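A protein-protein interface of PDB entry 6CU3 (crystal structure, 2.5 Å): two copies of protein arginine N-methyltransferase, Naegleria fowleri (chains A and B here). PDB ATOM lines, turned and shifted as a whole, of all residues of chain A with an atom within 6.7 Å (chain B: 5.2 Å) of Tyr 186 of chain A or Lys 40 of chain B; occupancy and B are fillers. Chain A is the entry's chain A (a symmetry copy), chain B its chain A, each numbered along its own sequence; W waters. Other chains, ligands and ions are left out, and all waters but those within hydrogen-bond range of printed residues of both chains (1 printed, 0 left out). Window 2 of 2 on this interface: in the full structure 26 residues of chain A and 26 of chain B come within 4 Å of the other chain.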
ATOM      1  N   PHE A 181       7.889 -11.540  24.330  1.00  0.00           N
ATOM      2  CA  PHE A 181       8.879 -10.486  24.499  1.00  0.00           C
ATOM      3  C   PHE A 181       9.464 -10.052  23.161  1.00  0.00           C
ATOM      4  O   PHE A 181       9.754  -8.865  22.963  1.00  0.00           O
ATOM      5  CB  PHE A 181       9.975 -10.993  25.453  1.00  0.00           C
ATOM      6  CG  PHE A 181      11.285 -10.282  25.328  1.00  0.00           C
ATOM      7  CD1 PHE A 181      11.511  -9.097  26.023  1.00  0.00           C
ATOM      8  CD2 PHE A 181      12.285 -10.780  24.491  1.00  0.00           C
ATOM      9  CE1 PHE A 181      12.722  -8.428  25.906  1.00  0.00           C
ATOM     10  CE2 PHE A 181      13.492 -10.112  24.349  1.00  0.00           C
ATOM     11  CZ  PHE A 181      13.719  -8.941  25.068  1.00  0.00           C
ATOM     12  N   ASN A 184       8.244  -6.869  20.642  1.00  0.00           N
ATOM     13  CA  ASN A 184       8.579  -5.451  20.862  1.00  0.00           C
ATOM     14  C   ASN A 184       9.848  -5.374  21.721  1.00  0.00           C
ATOM     15  O   ASN A 184       9.787  -5.305  22.951  1.00  0.00           O
ATOM     16  CB  ASN A 184       7.408  -4.735  21.523  1.00  0.00           C
ATOM     17  CG  ASN A 184       7.486  -3.225  21.401  1.00  0.00           C
ATOM     18  OD1 ASN A 184       8.564  -2.624  21.476  1.00  0.00           O
ATOM     19  ND2 ASN A 184       6.326  -2.593  21.245  1.00  0.00           N
ATOM     20  N   VAL A 185      10.998  -5.339  21.062  1.00  0.00           N
ATOM     21  CA  VAL A 185      12.291  -5.237  21.726  1.00  0.00           C
ATOM     22  C   VAL A 185      12.770  -3.797  21.557  1.00  0.00           C
ATOM     23  O   VAL A 185      13.320  -3.435  20.513  1.00  0.00           O
ATOM     24  CB  VAL A 185      13.287  -6.248  21.162  1.00  0.00           C
ATOM     25  CG1 VAL A 185      14.618  -6.142  21.875  1.00  0.00           C
ATOM     26  CG2 VAL A 185      12.719  -7.664  21.288  1.00  0.00           C
ATOM     27  N   TYR A 186      12.532  -2.974  22.590  1.00  0.00           N
ATOM     28  CA  TYR A 186      12.863  -1.547  22.587  1.00  0.00           C
ATOM     29  C   TYR A 186      12.264  -0.839  21.372  1.00  0.00           C
ATOM     30  O   TYR A 186      12.870   0.066  20.792  1.00  0.00           O
ATOM     31  CB  TYR A 186      14.380  -1.328  22.651  1.00  0.00           C
ATOM     32  CG  TYR A 186      15.018  -1.956  23.872  1.00  0.00           C
ATOM     33  CD1 TYR A 186      14.856  -1.383  25.137  1.00  0.00           C
ATOM     34  CD2 TYR A 186      15.774  -3.106  23.772  1.00  0.00           C
ATOM     35  CE1 TYR A 186      15.419  -1.941  26.263  1.00  0.00           C
ATOM     36  CE2 TYR A 186      16.336  -3.688  24.909  1.00  0.00           C
ATOM     37  CZ  TYR A 186      16.151  -3.098  26.152  1.00  0.00           C
ATOM     38  OH  TYR A 186      16.713  -3.662  27.279  1.00  0.00           O
ATOM     39  N   GLY A 187      11.048  -1.243  20.994  1.00  0.00           N
ATOM     40  CA  GLY A 187      10.381  -0.648  19.859  1.00  0.00           C
ATOM     41  C   GLY A 187      10.630  -1.368  18.555  1.00  0.00           C
ATOM     42  O   GLY A 187       9.999  -1.036  17.550  1.00  0.00           O
ATOM     43  N   PHE A 188      11.552  -2.317  18.526  1.00  0.00           N
ATOM     44  CA  PHE A 188      11.893  -3.005  17.298  1.00  0.00           C
ATOM     45  C   PHE A 188      11.161  -4.338  17.209  1.00  0.00           C
ATOM     46  O   PHE A 188      10.788  -4.943  18.220  1.00  0.00           O
ATOM     47  CB  PHE A 188      13.403  -3.206  17.195  1.00  0.00           C
ATOM     48  CG  PHE A 188      14.156  -1.926  17.039  1.00  0.00           C
ATOM     49  CD1 PHE A 188      14.052  -1.186  15.866  1.00  0.00           C
ATOM     50  CD2 PHE A 188      14.954  -1.441  18.067  1.00  0.00           C
ATOM     51  CE1 PHE A 188      14.756   0.006  15.730  1.00  0.00           C
ATOM     52  CE2 PHE A 188      15.659  -0.264  17.932  1.00  0.00           C
ATOM     53  CZ  PHE A 188      15.553   0.471  16.768  1.00  0.00           C
ATOM     54  N   ASP B  32      19.607  -9.442  28.503  1.00  0.00           N
ATOM     55  CA  ASP B  32      20.345  -8.821  29.610  1.00  0.00           C
ATOM     56  C   ASP B  32      19.918  -7.349  29.615  1.00  0.00           C
ATOM     57  O   ASP B  32      20.546  -6.497  28.973  1.00  0.00           O
ATOM     58  CB  ASP B  32      21.869  -8.991  29.466  1.00  0.00           C
ATOM     59  CG  ASP B  32      22.635  -8.580  30.728  1.00  0.00           C
ATOM     60  OD1 ASP B  32      22.043  -7.911  31.610  1.00  0.00           O
ATOM     61  OD2 ASP B  32      23.835  -8.918  30.834  1.00  0.00           O
ATOM     62  N   GLY B  33      18.860  -7.067  30.382  1.00  0.00           N
ATOM     63  CA  GLY B  33      18.285  -5.736  30.384  1.00  0.00           C
ATOM     64  C   GLY B  33      19.258  -4.676  30.850  1.00  0.00           C
ATOM     65  O   GLY B  33      19.385  -3.622  30.225  1.00  0.00           O
ATOM     66  N   THR B  36      21.761  -4.138  27.870  1.00  0.00           N
ATOM     67  CA  THR B  36      21.217  -3.499  26.686  1.00  0.00           C
ATOM     68  C   THR B  36      20.700  -2.094  26.991  1.00  0.00           C
ATOM     69  O   THR B  36      20.787  -1.196  26.144  1.00  0.00           O
ATOM     70  CB  THR B  36      20.133  -4.380  26.073  1.00  0.00           C
ATOM     71  OG1 THR B  36      20.692  -5.674  25.826  1.00  0.00           O
ATOM     72  CG2 THR B  36      19.662  -3.760  24.716  1.00  0.00           C
ATOM     73  N   ASN B  37      20.126  -1.887  28.176  1.00  0.00           N
ATOM     74  CA  ASN B  37      19.644  -0.560  28.505  1.00  0.00           C
ATOM     75  C   ASN B  37      20.785   0.449  28.526  1.00  0.00           C
ATOM     76  O   ASN B  37      20.620   1.593  28.073  1.00  0.00           O
ATOM     77  CB  ASN B  37      18.932  -0.580  29.852  1.00  0.00           C
ATOM     78  CG  ASN B  37      17.786   0.388  29.898  1.00  0.00           C
ATOM     79  OD1 ASN B  37      16.843   0.280  29.117  1.00  0.00           O
ATOM     80  ND2 ASN B  37      17.864   1.360  30.804  1.00  0.00           N
ATOM     81  N   ALA B  38      21.968   0.029  28.990  1.00  0.00           N
ATOM     82  CA  ALA B  38      23.106   0.941  29.002  1.00  0.00           C
ATOM     83  C   ALA B  38      23.526   1.308  27.584  1.00  0.00           C
ATOM     84  O   ALA B  38      23.700   2.487  27.268  1.00  0.00           O
ATOM     85  CB  ALA B  38      24.283   0.324  29.769  1.00  0.00           C
ATOM     86  N   TYR B  39      23.674   0.317  26.706  1.00  0.00           N
ATOM     87  CA  TYR B  39      24.026   0.647  25.326  1.00  0.00           C
ATOM     88  C   TYR B  39      22.962   1.534  24.687  1.00  0.00           C
ATOM     89  O   TYR B  39      23.292   2.467  23.949  1.00  0.00           O
ATOM     90  CB  TYR B  39      24.209  -0.617  24.495  1.00  0.00           C
ATOM     91  CG  TYR B  39      25.516  -1.344  24.702  1.00  0.00           C
ATOM     92  CD1 TYR B  39      25.713  -2.145  25.830  1.00  0.00           C
ATOM     93  CD2 TYR B  39      26.550  -1.247  23.770  1.00  0.00           C
ATOM     94  CE1 TYR B  39      26.896  -2.815  26.029  1.00  0.00           C
ATOM     95  CE2 TYR B  39      27.757  -1.922  23.961  1.00  0.00           C
ATOM     96  CZ  TYR B  39      27.911  -2.709  25.103  1.00  0.00           C
ATOM     97  OH  TYR B  39      29.082  -3.386  25.335  1.00  0.00           O
ATOM     98  N   LYS B  40      21.682   1.258  24.969  1.00  0.00           N
ATOM     99  CA  LYS B  40      20.594   2.020  24.370  1.00  0.00           C
ATOM    100  C   LYS B  40      20.686   3.497  24.742  1.00  0.00           C
ATOM    101  O   LYS B  40      20.552   4.371  23.882  1.00  0.00           O
ATOM    102  CB  LYS B  40      19.249   1.447  24.818  1.00  0.00           C
ATOM    103  CG  LYS B  40      18.063   2.026  24.077  1.00  0.00           C
ATOM    104  CD  LYS B  40      16.739   1.614  24.713  1.00  0.00           C
ATOM    105  CE  LYS B  40      16.713   1.946  26.202  1.00  0.00           C
ATOM    106  NZ  LYS B  40      16.032   3.237  26.475  1.00  0.00           N
ATOM    107  N   ASN B  41      20.936   3.786  26.016  1.00  0.00           N
ATOM    108  CA  ASN B  41      21.070   5.163  26.443  1.00  0.00           C
ATOM    109  C   ASN B  41      22.328   5.799  25.869  1.00  0.00           C
ATOM    110  O   ASN B  41      22.295   6.951  25.430  1.00  0.00           O
ATOM    111  CB  ASN B  41      21.047   5.223  27.970  1.00  0.00           C
ATOM    112  CG  ASN B  41      19.653   4.967  28.529  1.00  0.00           C
ATOM    113  OD1 ASN B  41      18.647   5.148  27.837  1.00  0.00           O
ATOM    114  ND2 ASN B  41      19.587   4.546  29.775  1.00  0.00           N
ATOM    115  N   ALA B  42      23.433   5.054  25.805  1.00  0.00           N
ATOM    116  CA  ALA B  42      24.659   5.645  25.278  1.00  0.00           C
ATOM    117  C   ALA B  42      24.500   6.067  23.828  1.00  0.00           C
ATOM    118  O   ALA B  42      25.088   7.067  23.409  1.00  0.00           O
ATOM    119  CB  ALA B  42      25.831   4.665  25.392  1.00  0.00           C
ATOM    120  N   ILE B  43      23.705   5.332  23.059  1.00  0.00           N
ATOM    121  CA  ILE B  43      23.562   5.576  21.632  1.00  0.00           C
ATOM    122  C   ILE B  43      22.402   6.541  21.395  1.00  0.00           C
ATOM    123  O   ILE B  43      22.603   7.622  20.829  1.00  0.00           O
ATOM    124  CB  ILE B  43      23.376   4.256  20.866  1.00  0.00           C
ATOM    125  CG1 ILE B  43      24.604   3.374  21.060  1.00  0.00           C
ATOM    126  CG2 ILE B  43      23.150   4.513  19.371  1.00  0.00           C
ATOM    127  CD1 ILE B  43      24.404   1.902  20.627  1.00  0.00           C
ATOM    128  N   LEU B  44      21.197   6.191  21.874  1.00  0.00           N
ATOM    129  CA  LEU B  44      20.011   6.973  21.520  1.00  0.00           C
ATOM    130  C   LEU B  44      19.953   8.316  22.241  1.00  0.00           C
ATOM    131  O   LEU B  44      19.282   9.229  21.752  1.00  0.00           O
ATOM    132  CB  LEU B  44      18.723   6.200  21.822  1.00  0.00           C
ATOM    133  CG  LEU B  44      18.493   4.932  20.994  1.00  0.00           C
ATOM    134  CD1 LEU B  44      17.078   4.402  21.158  1.00  0.00           C
ATOM    135  CD2 LEU B  44      18.840   5.153  19.520  1.00  0.00           C
ATOM    136  N   GLN B  45      20.662   8.476  23.363  1.00  0.00           N
ATOM    137  CA  GLN B  45      20.770   9.793  23.981  1.00  0.00           C
ATOM    138  C   GLN B  45      21.851  10.650  23.335  1.00  0.00           C
ATOM    139  O   GLN B  45      22.196  11.702  23.885  1.00  0.00           O
ATOM    140  CB  GLN B  45      21.088   9.696  25.472  1.00  0.00           C
ATOM    141  CG  GLN B  45      20.014   9.132  26.352  1.00  0.00           C
ATOM    142  CD  GLN B  45      20.508   8.981  27.777  1.00  0.00           C
ATOM    143  OE1 GLN B  45      21.686   9.251  28.084  1.00  0.00           O
ATOM    144  NE2 GLN B  45      19.622   8.543  28.656  1.00  0.00           N
ATOM    145  N   ILE B  64      20.578  -5.724  17.583  1.00  0.00           N
ATOM    146  CA  ILE B  64      19.880  -4.645  18.289  1.00  0.00           C
ATOM    147  C   ILE B  64      20.734  -3.367  18.368  1.00  0.00           C
ATOM    148  O   ILE B  64      20.215  -2.257  18.183  1.00  0.00           O
ATOM    149  CB  ILE B  64      19.443  -5.119  19.690  1.00  0.00           C
ATOM    150  CG1 ILE B  64      18.560  -4.070  20.369  1.00  0.00           C
ATOM    151  CG2 ILE B  64      20.664  -5.443  20.558  1.00  0.00           C
ATOM    152  CD1 ILE B  64      17.215  -3.844  19.724  1.00  0.00           C
ATOM    153  N   PHE B  68      19.976   0.429  17.122  1.00  0.00           N
ATOM    154  CA  PHE B  68      20.106   1.655  17.899  1.00  0.00           C
ATOM    155  C   PHE B  68      20.926   2.676  17.126  1.00  0.00           C
ATOM    156  O   PHE B  68      20.557   3.850  17.051  1.00  0.00           O
ATOM    157  CB  PHE B  68      20.765   1.392  19.257  1.00  0.00           C
ATOM    158  CG  PHE B  68      19.925   0.608  20.221  1.00  0.00           C
ATOM    159  CD1 PHE B  68      18.556   0.521  20.070  1.00  0.00           C
ATOM    160  CD2 PHE B  68      20.527  -0.049  21.299  1.00  0.00           C
ATOM    161  CE1 PHE B  68      17.787  -0.214  20.968  1.00  0.00           C
ATOM    162  CE2 PHE B  68      19.778  -0.783  22.202  1.00  0.00           C
ATOM    163  CZ  PHE B  68      18.398  -0.867  22.041  1.00  0.00           C
ATOM    164  N   LYS B  71      18.934   4.007  14.215  1.00  0.00           N
ATOM    165  CA  LYS B  71      17.895   4.895  14.708  1.00  0.00           C
ATOM    166  C   LYS B  71      18.479   6.201  15.244  1.00  0.00           C
ATOM    167  O   LYS B  71      17.816   7.242  15.196  1.00  0.00           O
ATOM    168  CB  LYS B  71      17.096   4.176  15.790  1.00  0.00           C
ATOM    169  CG  LYS B  71      15.862   4.919  16.259  1.00  0.00           C
ATOM    170  CD  LYS B  71      15.096   4.079  17.247  1.00  0.00           C
ATOM    171  CE  LYS B  71      14.563   4.897  18.395  1.00  0.00           C
ATOM    172  NZ  LYS B  71      13.252   4.344  18.849  1.00  0.00           N
HETATM  173  O   HOH W   1      14.314   2.427  20.592  1.00  0.00           O
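Water W1 bridges the backbone carbonyl oxygen (O) of Tyr 186 of chain A and the side-chain amino group (NZ) of Lys 71 of chain B.
O of Asp 32 of chain B lies within hydrogen-bond range of OG1 of Thr 36 of chain B (3.3 Å).
Among the printed residues, pairs that only touch across the chains: Val 185 of chain A with Ile 64 of chain B (3.995 Å), Tyr 186 of chain A with Gly 33 of chain B (3.98 Å), Tyr 186 of chain A with Thr 36 of chain B (3.3 Å), Tyr 186 of chain A with Asn 37 of chain B (3.9 Å), Tyr 186 of chain A with Lys 40 of chain B (3.6 Å), Tyr 186 of chain A with Phe 68 of chain B (3.9 Å), Phe 188 of chain A with Ile 64 of chain B (3.7 Å), Phe 188 of chain A with Phe 68 of chain B (3.7 Å) and Phe 188 of chain A with Lys 71 of chain B (3.7 Å).
No position is printed for both chains.
Of the 9 pairs that touch across the chains among the printed residues, none has its exchanged pair printed and touching as well.
Hydrophobic or aromatic side chains of chain B within 4 Å of the printed part of chain A: Ile 64 and Phe 68.
Of the 6 printed residues of chain A, 3 touch a printed residue of chain B.
Among the printed residues, 9 pairs touch across the chains.
Among the printed residues, no Asp or Glu carboxylate lies within 4 Å of a Lys or Arg side-chain nitrogen of the other chain.
Lys 40 of chain B touches one residue of chain A.
Of the printed residues of chain A, Gly 33 of chain B touches Tyr 186 (3.98 Å).
Of the printed residues of chain A, Ile 64 of chain B touches Val 185 and Phe 188.
Of the printed residues of chain A, Lys 71 of chain B touches Phe 188.
The nearest printed residue of chain A that does not touch Phe 68 of chain B is Val 185 of chain A (5.5 Å).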
